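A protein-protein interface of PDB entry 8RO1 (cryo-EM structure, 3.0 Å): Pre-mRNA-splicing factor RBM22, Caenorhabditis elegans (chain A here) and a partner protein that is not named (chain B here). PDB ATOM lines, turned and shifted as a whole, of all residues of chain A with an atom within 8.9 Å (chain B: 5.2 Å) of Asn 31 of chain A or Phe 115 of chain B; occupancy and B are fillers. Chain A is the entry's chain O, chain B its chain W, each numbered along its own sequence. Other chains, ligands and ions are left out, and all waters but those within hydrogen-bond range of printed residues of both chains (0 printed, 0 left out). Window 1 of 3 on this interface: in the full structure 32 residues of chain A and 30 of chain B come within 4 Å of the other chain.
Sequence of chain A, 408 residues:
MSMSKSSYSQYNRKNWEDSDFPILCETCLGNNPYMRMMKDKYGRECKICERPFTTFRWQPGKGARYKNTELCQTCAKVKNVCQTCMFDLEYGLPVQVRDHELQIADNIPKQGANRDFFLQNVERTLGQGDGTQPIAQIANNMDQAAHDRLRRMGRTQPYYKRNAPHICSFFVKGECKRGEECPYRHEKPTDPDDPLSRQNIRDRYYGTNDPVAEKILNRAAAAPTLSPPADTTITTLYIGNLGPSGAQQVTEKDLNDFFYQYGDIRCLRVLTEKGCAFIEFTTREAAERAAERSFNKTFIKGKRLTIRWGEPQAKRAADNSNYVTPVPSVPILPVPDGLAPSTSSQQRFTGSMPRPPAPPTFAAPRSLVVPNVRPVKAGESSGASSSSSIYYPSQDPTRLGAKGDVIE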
ATOM      1  N   CYS A  25     -10.126 -22.305  12.221  1.00  0.00           N
ATOM      2  CA  CYS A  25     -11.261 -22.811  11.470  1.00  0.00           C
ATOM      3  C   CYS A  25     -11.219 -22.331  10.026  1.00  0.00           C
ATOM      4  O   CYS A  25     -10.175 -21.876   9.555  1.00  0.00           O
ATOM      5  CB  CYS A  25     -12.543 -22.353  12.170  1.00  0.00           C
ATOM      6  SG  CYS A  25     -12.639 -20.586  12.427  1.00  0.00           S
ATOM      7  N   GLU A  26     -12.347 -22.396   9.318  1.00  0.00           N
ATOM      8  CA  GLU A  26     -12.474 -21.806   7.995  1.00  0.00           C
ATOM      9  C   GLU A  26     -12.851 -20.343   8.011  1.00  0.00           C
ATOM     10  O   GLU A  26     -12.459 -19.624   7.108  1.00  0.00           O
ATOM     11  CB  GLU A  26     -13.451 -22.605   7.142  1.00  0.00           C
ATOM     12  CG  GLU A  26     -13.021 -24.056   6.918  1.00  0.00           C
ATOM     13  CD  GLU A  26     -11.655 -24.187   6.261  1.00  0.00           C
ATOM     14  OE1 GLU A  26     -11.406 -23.470   5.276  1.00  0.00           O
ATOM     15  OE2 GLU A  26     -10.822 -24.974   6.746  1.00  0.00           O
ATOM     16  N   THR A  27     -13.611 -19.867   8.992  1.00  0.00           N
ATOM     17  CA  THR A  27     -14.067 -18.484   8.897  1.00  0.00           C
ATOM     18  C   THR A  27     -12.917 -17.509   9.025  1.00  0.00           C
ATOM     19  O   THR A  27     -12.959 -16.431   8.427  1.00  0.00           O
ATOM     20  CB  THR A  27     -15.103 -18.130   9.962  1.00  0.00           C
ATOM     21  OG1 THR A  27     -14.436 -17.879  11.200  1.00  0.00           O
ATOM     22  CG2 THR A  27     -16.157 -19.211  10.154  1.00  0.00           C
ATOM     23  N   CYS A  28     -11.889 -17.866   9.783  1.00  0.00           N
ATOM     24  CA  CYS A  28     -10.734 -16.995   9.929  1.00  0.00           C
ATOM     25  C   CYS A  28      -9.883 -16.985   8.673  1.00  0.00           C
ATOM     26  O   CYS A  28      -9.512 -15.922   8.183  1.00  0.00           O
ATOM     27  CB  CYS A  28      -9.907 -17.407  11.134  1.00  0.00           C
ATOM     28  SG  CYS A  28     -10.824 -17.350  12.651  1.00  0.00           S
ATOM     29  N   LEU A  29      -9.568 -18.153   8.136  1.00  0.00           N
ATOM     30  CA  LEU A  29      -8.863 -18.288   6.862  1.00  0.00           C
ATOM     31  C   LEU A  29      -9.692 -17.995   5.611  1.00  0.00           C
ATOM     32  O   LEU A  29      -9.122 -17.653   4.576  1.00  0.00           O
ATOM     33  CB  LEU A  29      -8.411 -19.731   6.698  1.00  0.00           C
ATOM     34  CG  LEU A  29      -7.183 -20.335   7.332  1.00  0.00           C
ATOM     35  CD1 LEU A  29      -7.224 -20.132   8.785  1.00  0.00           C
ATOM     36  CD2 LEU A  29      -7.144 -21.808   7.037  1.00  0.00           C
ATOM     37  N   GLY A  30     -11.007 -18.073   5.689  1.00  0.00           N
ATOM     38  CA  GLY A  30     -11.818 -18.539   4.572  1.00  0.00           C
ATOM     39  C   GLY A  30     -11.807 -18.240   3.092  1.00  0.00           C
ATOM     40  O   GLY A  30     -11.645 -19.211   2.348  1.00  0.00           O
ATOM     41  N   ASN A  31     -11.966 -17.016   2.609  1.00  0.00           N
ATOM     42  CA  ASN A  31     -12.571 -16.906   1.277  1.00  0.00           C
ATOM     43  C   ASN A  31     -11.652 -17.378   0.155  1.00  0.00           C
ATOM     44  O   ASN A  31     -12.145 -17.952  -0.821  1.00  0.00           O
ATOM     45  CB  ASN A  31     -13.059 -15.482   1.003  1.00  0.00           C
ATOM     46  CG  ASN A  31     -12.010 -14.428   1.273  1.00  0.00           C
ATOM     47  OD1 ASN A  31     -11.123 -14.192   0.452  1.00  0.00           O
ATOM     48  ND2 ASN A  31     -12.105 -13.788   2.431  1.00  0.00           N
ATOM     49  N   ASN A  32     -10.337 -17.215   0.292  1.00  0.00           N
ATOM     50  CA  ASN A  32      -9.409 -17.464  -0.806  1.00  0.00           C
ATOM     51  C   ASN A  32      -8.674 -18.781  -0.558  1.00  0.00           C
ATOM     52  O   ASN A  32      -8.097 -18.945   0.520  1.00  0.00           O
ATOM     53  CB  ASN A  32      -8.431 -16.285  -0.876  1.00  0.00           C
ATOM     54  CG  ASN A  32      -7.411 -16.381  -1.989  1.00  0.00           C
ATOM     55  OD1 ASN A  32      -7.259 -17.396  -2.659  1.00  0.00           O
ATOM     56  ND2 ASN A  32      -6.707 -15.287  -2.197  1.00  0.00           N
ATOM     57  N   PRO A  33      -8.637 -19.727  -1.505  1.00  0.00           N
ATOM     58  CA  PRO A  33      -7.896 -20.972  -1.272  1.00  0.00           C
ATOM     59  C   PRO A  33      -6.413 -20.798  -1.088  1.00  0.00           C
ATOM     60  O   PRO A  33      -5.765 -21.710  -0.567  1.00  0.00           O
ATOM     61  CB  PRO A  33      -8.163 -21.787  -2.535  1.00  0.00           C
ATOM     62  CG  PRO A  33      -9.323 -21.257  -3.103  1.00  0.00           C
ATOM     63  CD  PRO A  33      -9.343 -19.806  -2.786  1.00  0.00           C
ATOM     64  N   TYR A  34      -5.852 -19.673  -1.516  1.00  0.00           N
ATOM     65  CA  TYR A  34      -4.420 -19.434  -1.523  1.00  0.00           C
ATOM     66  C   TYR A  34      -4.105 -18.389  -0.475  1.00  0.00           C
ATOM     67  O   TYR A  34      -4.800 -17.375  -0.379  1.00  0.00           O
ATOM     68  CB  TYR A  34      -3.972 -18.914  -2.876  1.00  0.00           C
ATOM     69  CG  TYR A  34      -4.137 -19.854  -4.017  1.00  0.00           C
ATOM     70  CD1 TYR A  34      -3.167 -20.761  -4.350  1.00  0.00           C
ATOM     71  CD2 TYR A  34      -5.270 -19.808  -4.780  1.00  0.00           C
ATOM     72  CE1 TYR A  34      -3.347 -21.602  -5.393  1.00  0.00           C
ATOM     73  CE2 TYR A  34      -5.454 -20.646  -5.811  1.00  0.00           C
ATOM     74  CZ  TYR A  34      -4.495 -21.529  -6.128  1.00  0.00           C
ATOM     75  OH  TYR A  34      -4.690 -22.341  -7.209  1.00  0.00           O
ATOM     76  N   MET A  35      -3.045 -18.612   0.288  1.00  0.00           N
ATOM     77  CA  MET A  35      -2.740 -17.762   1.423  1.00  0.00           C
ATOM     78  C   MET A  35      -1.250 -17.574   1.571  1.00  0.00           C
ATOM     79  O   MET A  35      -0.465 -18.470   1.284  1.00  0.00           O
ATOM     80  CB  MET A  35      -3.244 -18.382   2.717  1.00  0.00           C
ATOM     81  CG  MET A  35      -4.690 -18.744   2.737  1.00  0.00           C
ATOM     82  SD  MET A  35      -5.158 -19.321   4.350  1.00  0.00           S
ATOM     83  CE  MET A  35      -5.263 -17.763   5.219  1.00  0.00           C
ATOM     84  N   TRP A  58      -1.824 -13.767   9.212  1.00  0.00           N
ATOM     85  CA  TRP A  58      -2.297 -13.895   7.842  1.00  0.00           C
ATOM     86  C   TRP A  58      -3.375 -12.854   7.619  1.00  0.00           C
ATOM     87  O   TRP A  58      -4.013 -12.407   8.570  1.00  0.00           O
ATOM     88  CB  TRP A  58      -2.831 -15.300   7.560  1.00  0.00           C
ATOM     89  CG  TRP A  58      -4.029 -15.612   8.324  1.00  0.00           C
ATOM     90  CD1 TRP A  58      -5.302 -15.517   7.908  1.00  0.00           C
ATOM     91  CD2 TRP A  58      -4.076 -16.046   9.665  1.00  0.00           C
ATOM     92  NE1 TRP A  58      -6.151 -15.887   8.901  1.00  0.00           N
ATOM     93  CE2 TRP A  58      -5.414 -16.177  10.012  1.00  0.00           C
ATOM     94  CE3 TRP A  58      -3.107 -16.355  10.604  1.00  0.00           C
ATOM     95  CZ2 TRP A  58      -5.807 -16.570  11.259  1.00  0.00           C
ATOM     96  CZ3 TRP A  58      -3.496 -16.726  11.830  1.00  0.00           C
ATOM     97  CH2 TRP A  58      -4.827 -16.839  12.154  1.00  0.00           C
ATOM     98  N   GLN A  59      -3.543 -12.439   6.365  1.00  0.00           N
ATOM     99  CA  GLN A  59      -4.669 -11.603   5.965  1.00  0.00           C
ATOM    100  C   GLN A  59      -5.619 -12.484   5.175  1.00  0.00           C
ATOM    101  O   GLN A  59      -5.270 -12.893   4.062  1.00  0.00           O
ATOM    102  CB  GLN A  59      -4.235 -10.415   5.112  1.00  0.00           C
ATOM    103  CG  GLN A  59      -5.391  -9.502   4.717  1.00  0.00           C
ATOM    104  CD  GLN A  59      -4.975  -8.381   3.824  1.00  0.00           C
ATOM    105  OE1 GLN A  59      -4.141  -8.558   2.945  1.00  0.00           O
ATOM    106  NE2 GLN A  59      -5.536  -7.208   4.051  1.00  0.00           N
ATOM    107  N   PRO A  60      -6.814 -12.780   5.654  1.00  0.00           N
ATOM    108  CA  PRO A  60      -7.673 -13.688   4.898  1.00  0.00           C
ATOM    109  C   PRO A  60      -8.436 -13.028   3.758  1.00  0.00           C
ATOM    110  O   PRO A  60      -9.614 -12.710   3.830  1.00  0.00           O
ATOM    111  CB  PRO A  60      -8.605 -14.226   5.976  1.00  0.00           C
ATOM    112  CG  PRO A  60      -8.711 -13.174   6.906  1.00  0.00           C
ATOM    113  CD  PRO A  60      -7.391 -12.533   6.979  1.00  0.00           C
ATOM    114  N   GLY A  61      -7.711 -12.810   2.674  1.00  0.00           N
ATOM    115  CA  GLY A  61      -8.273 -12.271   1.459  1.00  0.00           C
ATOM    116  C   GLY A  61      -8.423 -10.775   1.482  1.00  0.00           C
ATOM    117  O   GLY A  61      -8.086 -10.087   2.444  1.00  0.00           O
ATOM    118  N   LYS A  62      -8.930 -10.274   0.357  1.00  0.00           N
ATOM    119  CA  LYS A  62      -9.200  -8.856   0.173  1.00  0.00           C
ATOM    120  C   LYS A  62     -10.034  -8.288   1.309  1.00  0.00           C
ATOM    121  O   LYS A  62     -11.005  -8.897   1.758  1.00  0.00           O
ATOM    122  CB  LYS A  62      -9.924  -8.669  -1.162  1.00  0.00           C
ATOM    123  CG  LYS A  62     -10.443  -7.272  -1.474  1.00  0.00           C
ATOM    124  CD  LYS A  62     -11.031  -7.242  -2.876  1.00  0.00           C
ATOM    125  CE  LYS A  62     -11.941  -6.048  -3.101  1.00  0.00           C
ATOM    126  NZ  LYS A  62     -11.201  -4.763  -3.104  1.00  0.00           N
ATOM    127  N   GLY A  63      -9.622  -7.118   1.781  1.00  0.00           N
ATOM    128  CA  GLY A  63     -10.377  -6.338   2.729  1.00  0.00           C
ATOM    129  C   GLY A  63     -10.278  -6.782   4.168  1.00  0.00           C
ATOM    130  O   GLY A  63     -10.643  -6.009   5.058  1.00  0.00           O
ATOM    131  N   ALA A  64      -9.771  -7.976   4.442  1.00  0.00           N
ATOM    132  CA  ALA A  64      -9.572  -8.372   5.819  1.00  0.00           C
ATOM    133  C   ALA A  64      -8.398  -7.634   6.441  1.00  0.00           C
ATOM    134  O   ALA A  64      -7.550  -7.063   5.756  1.00  0.00           O
ATOM    135  CB  ALA A  64      -9.356  -9.872   5.900  1.00  0.00           C
ATOM    136  N   PRO A 158     -19.811 -19.515   6.732  1.00  0.00           N
ATOM    137  CA  PRO A 158     -18.825 -18.695   7.442  1.00  0.00           C
ATOM    138  C   PRO A 158     -19.190 -17.223   7.408  1.00  0.00           C
ATOM    139  O   PRO A 158     -19.678 -16.709   6.400  1.00  0.00           O
ATOM    140  CB  PRO A 158     -17.524 -18.965   6.682  1.00  0.00           C
ATOM    141  CG  PRO A 158     -17.939 -19.284   5.344  1.00  0.00           C
ATOM    142  CD  PRO A 158     -19.239 -20.008   5.466  1.00  0.00           C
ATOM    143  N   TYR A 159     -18.943 -16.545   8.522  1.00  0.00           N
ATOM    144  CA  TYR A 159     -19.281 -15.136   8.704  1.00  0.00           C
ATOM    145  C   TYR A 159     -17.977 -14.343   8.622  1.00  0.00           C
ATOM    146  O   TYR A 159     -17.275 -14.173   9.618  1.00  0.00           O
ATOM    147  CB  TYR A 159     -20.027 -14.951  10.025  1.00  0.00           C
ATOM    148  CG  TYR A 159     -20.482 -13.549  10.352  1.00  0.00           C
ATOM    149  CD1 TYR A 159     -21.165 -12.792   9.418  1.00  0.00           C
ATOM    150  CD2 TYR A 159     -20.320 -13.020  11.616  1.00  0.00           C
ATOM    151  CE1 TYR A 159     -21.628 -11.545   9.709  1.00  0.00           C
ATOM    152  CE2 TYR A 159     -20.785 -11.763  11.909  1.00  0.00           C
ATOM    153  CZ  TYR A 159     -21.436 -11.031  10.959  1.00  0.00           C
ATOM    154  OH  TYR A 159     -21.873  -9.759  11.259  1.00  0.00           O
ATOM    155  N   TYR A 160     -17.656 -13.862   7.417  1.00  0.00           N
ATOM    156  CA  TYR A 160     -16.418 -13.113   7.190  1.00  0.00           C
ATOM    157  C   TYR A 160     -16.435 -11.715   7.797  1.00  0.00           C
ATOM    158  O   TYR A 160     -15.363 -11.150   8.035  1.00  0.00           O
ATOM    159  CB  TYR A 160     -16.107 -13.040   5.695  1.00  0.00           C
ATOM    160  CG  TYR A 160     -15.932 -14.386   5.032  1.00  0.00           C
ATOM    161  CD1 TYR A 160     -15.162 -15.372   5.619  1.00  0.00           C
ATOM    162  CD2 TYR A 160     -16.520 -14.667   3.816  1.00  0.00           C
ATOM    163  CE1 TYR A 160     -14.990 -16.578   5.039  1.00  0.00           C
ATOM    164  CE2 TYR A 160     -16.343 -15.884   3.218  1.00  0.00           C
ATOM    165  CZ  TYR A 160     -15.580 -16.837   3.839  1.00  0.00           C
ATOM    166  OH  TYR A 160     -15.401 -18.070   3.263  1.00  0.00           O
ATOM    167  N   LYS A 161     -17.603 -11.087   7.923  1.00  0.00           N
ATOM    168  CA  LYS A 161     -17.655  -9.731   8.461  1.00  0.00           C
ATOM    169  C   LYS A 161     -17.016  -9.678   9.844  1.00  0.00           C
ATOM    170  O   LYS A 161     -16.307  -8.722  10.170  1.00  0.00           O
ATOM    171  CB  LYS A 161     -19.098  -9.239   8.514  1.00  0.00           C
ATOM    172  CG  LYS A 161     -19.259  -7.780   8.924  1.00  0.00           C
ATOM    173  CD  LYS A 161     -20.729  -7.340   8.993  1.00  0.00           C
ATOM    174  CE  LYS A 161     -21.418  -7.227   7.635  1.00  0.00           C
ATOM    175  NZ  LYS A 161     -21.006  -6.004   6.899  1.00  0.00           N
ATOM    176  N   ASN A 163     -14.682 -11.798  10.782  1.00  0.00           N
ATOM    177  CA  ASN A 163     -13.257 -11.967  10.529  1.00  0.00           C
ATOM    178  C   ASN A 163     -12.584 -10.623  10.209  1.00  0.00           C
ATOM    179  O   ASN A 163     -11.546 -10.294  10.784  1.00  0.00           O
ATOM    180  CB  ASN A 163     -13.137 -13.040   9.424  1.00  0.00           C
ATOM    181  CG  ASN A 163     -11.819 -13.104   8.666  1.00  0.00           C
ATOM    182  OD1 ASN A 163     -11.106 -12.142   8.403  1.00  0.00           O
ATOM    183  ND2 ASN A 163     -11.541 -14.316   8.227  1.00  0.00           N
ATOM    184  N   ALA A 164     -13.160  -9.828   9.296  1.00  0.00           N
ATOM    185  CA  ALA A 164     -12.296  -8.956   8.496  1.00  0.00           C
ATOM    186  C   ALA A 164     -11.665  -7.713   9.149  1.00  0.00           C
ATOM    187  O   ALA A 164     -10.426  -7.667   9.189  1.00  0.00           O
ATOM    188  CB  ALA A 164     -13.000  -8.647   7.167  1.00  0.00           C
ATOM    189  N   GLN B 111      -2.209 -16.962  -8.982  1.00  0.00           N
ATOM    190  CA  GLN B 111      -3.519 -17.430  -8.544  1.00  0.00           C
ATOM    191  C   GLN B 111      -4.076 -16.695  -7.317  1.00  0.00           C
ATOM    192  O   GLN B 111      -5.298 -16.604  -7.190  1.00  0.00           O
ATOM    193  CB  GLN B 111      -3.479 -18.928  -8.277  1.00  0.00           C
ATOM    194  CG  GLN B 111      -3.028 -19.768  -9.453  1.00  0.00           C
ATOM    195  CD  GLN B 111      -3.926 -19.615 -10.645  1.00  0.00           C
ATOM    196  OE1 GLN B 111      -5.099 -19.310 -10.503  1.00  0.00           O
ATOM    197  NE2 GLN B 111      -3.386 -19.837 -11.831  1.00  0.00           N
ATOM    198  N   ILE B 112      -3.248 -16.197  -6.387  1.00  0.00           N
ATOM    199  CA  ILE B 112      -3.773 -15.280  -5.366  1.00  0.00           C
ATOM    200  C   ILE B 112      -4.420 -14.073  -6.017  1.00  0.00           C
ATOM    201  O   ILE B 112      -5.553 -13.694  -5.701  1.00  0.00           O
ATOM    202  CB  ILE B 112      -2.661 -14.847  -4.381  1.00  0.00           C
ATOM    203  CG1 ILE B 112      -2.309 -15.999  -3.438  1.00  0.00           C
ATOM    204  CG2 ILE B 112      -3.009 -13.484  -3.622  1.00  0.00           C
ATOM    205  CD1 ILE B 112      -1.479 -15.670  -2.213  1.00  0.00           C
ATOM    206  N   ARG B 113      -3.688 -13.444  -6.912  1.00  0.00           N
ATOM    207  CA  ARG B 113      -4.023 -12.131  -7.444  1.00  0.00           C
ATOM    208  C   ARG B 113      -5.307 -12.188  -8.254  1.00  0.00           C
ATOM    209  O   ARG B 113      -6.046 -11.203  -8.315  1.00  0.00           O
ATOM    210  CB  ARG B 113      -2.813 -11.646  -8.218  1.00  0.00           C
ATOM    211  CG  ARG B 113      -1.766 -11.224  -7.209  1.00  0.00           C
ATOM    212  CD  ARG B 113      -0.387 -11.143  -7.776  1.00  0.00           C
ATOM    213  NE  ARG B 113       0.593 -10.867  -6.730  1.00  0.00           N
ATOM    214  CZ  ARG B 113       1.851 -10.490  -6.928  1.00  0.00           C
ATOM    215  NH1 ARG B 113       2.658 -10.361  -5.884  1.00  0.00           N
ATOM    216  NH2 ARG B 113       2.344 -10.324  -8.139  1.00  0.00           N
ATOM    217  N   SER B 114      -5.585 -13.331  -8.874  1.00  0.00           N
ATOM    218  CA  SER B 114      -6.802 -13.497  -9.651  1.00  0.00           C
ATOM    219  C   SER B 114      -7.999 -13.667  -8.734  1.00  0.00           C
ATOM    220  O   SER B 114      -9.054 -13.081  -8.988  1.00  0.00           O
ATOM    221  CB  SER B 114      -6.689 -14.707 -10.566  1.00  0.00           C
ATOM    222  OG  SER B 114      -6.332 -15.847  -9.825  1.00  0.00           O
ATOM    223  N   PHE B 115      -7.866 -14.458  -7.674  1.00  0.00           N
ATOM    224  CA  PHE B 115      -8.973 -14.589  -6.735  1.00  0.00           C
ATOM    225  C   PHE B 115      -9.258 -13.265  -6.057  1.00  0.00           C
ATOM    226  O   PHE B 115     -10.418 -12.904  -5.849  1.00  0.00           O
ATOM    227  CB  PHE B 115      -8.656 -15.640  -5.677  1.00  0.00           C
ATOM    228  CG  PHE B 115      -9.865 -16.258  -5.050  1.00  0.00           C
ATOM    229  CD1 PHE B 115     -10.555 -15.576  -4.078  1.00  0.00           C
ATOM    230  CD2 PHE B 115     -10.323 -17.490  -5.432  1.00  0.00           C
ATOM    231  CE1 PHE B 115     -11.673 -16.101  -3.513  1.00  0.00           C
ATOM    232  CE2 PHE B 115     -11.433 -18.031  -4.859  1.00  0.00           C
ATOM    233  CZ  PHE B 115     -12.116 -17.328  -3.899  1.00  0.00           C
ATOM    234  N   ASP B 116      -8.216 -12.549  -5.674  1.00  0.00           N
ATOM    235  CA  ASP B 116      -8.418 -11.314  -4.939  1.00  0.00           C
ATOM    236  C   ASP B 116      -9.041 -10.247  -5.829  1.00  0.00           C
ATOM    237  O   ASP B 116     -10.056  -9.643  -5.474  1.00  0.00           O
ATOM    238  CB  ASP B 116      -7.080 -10.842  -4.383  1.00  0.00           C
ATOM    239  CG  ASP B 116      -6.595 -11.700  -3.231  1.00  0.00           C
ATOM    240  OD1 ASP B 116      -7.349 -12.577  -2.765  1.00  0.00           O
ATOM    241  OD2 ASP B 116      -5.442 -11.506  -2.797  1.00  0.00           O
ATOM    242  N   THR B 117      -8.444 -10.004  -6.998  1.00  0.00           N
ATOM    243  CA  THR B 117      -8.930  -8.933  -7.864  1.00  0.00           C
ATOM    244  C   THR B 117     -10.226  -9.302  -8.572  1.00  0.00           C
ATOM    245  O   THR B 117     -11.095  -8.443  -8.750  1.00  0.00           O
ATOM    246  CB  THR B 117      -7.862  -8.538  -8.883  1.00  0.00           C
ATOM    247  OG1 THR B 117      -7.519  -9.675  -9.679  1.00  0.00           O
ATOM    248  CG2 THR B 117      -6.615  -7.997  -8.191  1.00  0.00           C
ATOM    249  N   LEU B 118     -10.388 -10.565  -8.969  1.00  0.00           N
ATOM    250  CA  LEU B 118     -11.416 -10.951  -9.931  1.00  0.00           C
ATOM    251  C   LEU B 118     -12.520 -11.795  -9.327  1.00  0.00           C
ATOM    252  O   LEU B 118     -13.626 -11.799  -9.865  1.00  0.00           O
ATOM    253  CB  LEU B 118     -10.820 -11.713 -11.119  1.00  0.00           C
ATOM    254  CG  LEU B 118      -9.531 -11.224 -11.765  1.00  0.00           C
ATOM    255  CD1 LEU B 118      -9.157 -12.141 -12.906  1.00  0.00           C
ATOM    256  CD2 LEU B 118      -9.631  -9.799 -12.250  1.00  0.00           C
ATOM    257  N   GLY B 119     -12.246 -12.530  -8.257  1.00  0.00           N
ATOM    258  CA  GLY B 119     -13.216 -13.421  -7.664  1.00  0.00           C
ATOM    259  C   GLY B 119     -13.108 -14.867  -8.059  1.00  0.00           C
ATOM    260  O   GLY B 119     -13.995 -15.646  -7.702  1.00  0.00           O
ATOM    261  N   TYR B 120     -12.050 -15.268  -8.753  1.00  0.00           N
ATOM    262  CA  TYR B 120     -11.961 -16.664  -9.139  1.00  0.00           C
ATOM    263  C   TYR B 120     -10.524 -17.037  -9.436  1.00  0.00           C
ATOM    264  O   TYR B 120      -9.677 -16.191  -9.723  1.00  0.00           O
ATOM    265  CB  TYR B 120     -12.856 -16.946 -10.344  1.00  0.00           C
ATOM    266  CG  TYR B 120     -12.538 -16.117 -11.558  1.00  0.00           C
ATOM    267  CD1 TYR B 120     -11.616 -16.549 -12.482  1.00  0.00           C
ATOM    268  CD2 TYR B 120     -13.167 -14.911 -11.782  1.00  0.00           C
ATOM    269  CE1 TYR B 120     -11.324 -15.817 -13.597  1.00  0.00           C
ATOM    270  CE2 TYR B 120     -12.878 -14.165 -12.898  1.00  0.00           C
ATOM    271  CZ  TYR B 120     -11.945 -14.619 -13.797  1.00  0.00           C
ATOM    272  OH  TYR B 120     -11.646 -13.887 -14.919  1.00  0.00           O
ATOM    273  N   ALA B 121     -10.282 -18.336  -9.374  1.00  0.00           N
ATOM    274  CA  ALA B 121      -8.957 -18.915  -9.354  1.00  0.00           C
ATOM    275  C   ALA B 121      -9.053 -20.304  -9.938  1.00  0.00           C
ATOM    276  O   ALA B 121     -10.128 -20.902  -9.983  1.00  0.00           O
ATOM    277  CB  ALA B 121      -8.367 -18.973  -7.952  1.00  0.00           C
ATOM    278  N   VAL B 134     -12.460 -22.191  -9.432  1.00  0.00           N
ATOM    279  CA  VAL B 134     -13.194 -21.968  -8.183  1.00  0.00           C
ATOM    280  C   VAL B 134     -13.438 -20.480  -7.997  1.00  0.00           C
ATOM    281  O   VAL B 134     -12.498 -19.717  -7.761  1.00  0.00           O
ATOM    282  CB  VAL B 134     -12.479 -22.548  -6.958  1.00  0.00           C
ATOM    283  CG1 VAL B 134     -12.521 -24.056  -6.995  1.00  0.00           C
ATOM    284  CG2 VAL B 134     -11.045 -22.087  -6.818  1.00  0.00           C
ATOM    285  N   GLY B 135     -14.689 -20.060  -8.105  1.00  0.00           N
ATOM    286  CA  GLY B 135     -15.012 -18.672  -7.821  1.00  0.00           C
ATOM    287  C   GLY B 135     -16.385 -18.307  -8.330  1.00  0.00           C
ATOM    288  O   GLY B 135     -17.266 -19.160  -8.468  1.00  0.00           O
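The side-chain amide nitrogen (ND2) of Asn 32 of chain A is in hydrogen-bond range of the side-chain carboxylate (OD1) of Asp 116 of chain B, 2.8 Å away.
The backbone carbonyl oxygen of Ala 121 of chain B sits at hydrogen-bond distance from the backbone NH of Val 134 of chain B, at 2.7 Å. The side-chain amide oxygen (OD1) of Asn 32 of chain A sits at hydrogen-bond distance from the backbone NH (N) of Tyr 34 of chain A. N of Phe 115 of chain B sits at hydrogen-bond distance from O of Tyr 120 of chain B (3.2 Å). ND2 of Asn 31 of chain A lies within hydrogen-bond range of O of Pro 60 of chain A (3.1 Å). OG of Ser 114 of chain B sits at hydrogen-bond distance from O of Gln 111 of chain B (2.9 Å).
Among the printed residues, pairs that only touch across the chains: Asn 31 of chain A with Phe 115 of chain B, Asn 32 of chain A with Phe 115 of chain B, Pro 33 of chain A with Phe 115 of chain B, Tyr 34 of chain A with Gln 111 of chain B, Tyr 34 of chain A with Ile 112 of chain B, Tyr 34 of chain A with Ala 121 of chain B and Lys 62 of chain A with Asp 116 of chain B.
Printed residues of chain B within 4 Å of Asn 31 of chain A: Phe 115 (3.1 Å). Of chain A, only Asn 31 (3.1 Å), Asn 32 (3.7 Å) and Pro 33 (3.4 Å) come within 4 Å of Phe 115 of chain B. No residue of chain A comes within 4 Å of Ser 114 of chain B. Of the printed residues of chain A, Asp 116 of chain B touches Asn 32 and Lys 62. Printed residues of chain B within 4 Å of Lys 62 of chain A: Asp 116. Of the printed residues of chain A, Ile 112 of chain B touches Tyr 34 (3.4 Å). Printed residues of chain A within 4 Å of Ala 121 of chain B: Tyr 34 (3.98 Å). Lys 161 of chain A touches none of the printed residues of chain B. The nearest printed residue of chain B that does not touch Asn 31 of chain A is Asp 116 of chain B (5.2 Å). The nearest printed residue of chain B that does not touch Lys 62 of chain A is Thr 117 of chain B (5.6 Å).
Printed residues of chain A that touch a printed residue of chain B: Asn 31, Asn 32, Pro 33, Tyr 34 and Lys 62. Among the printed residues, 8 pairs touch across the chains. Among the printed residues, no Asp or Glu carboxylate lies within 4 Å of a Lys or Arg side-chain nitrogen of the other chain.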
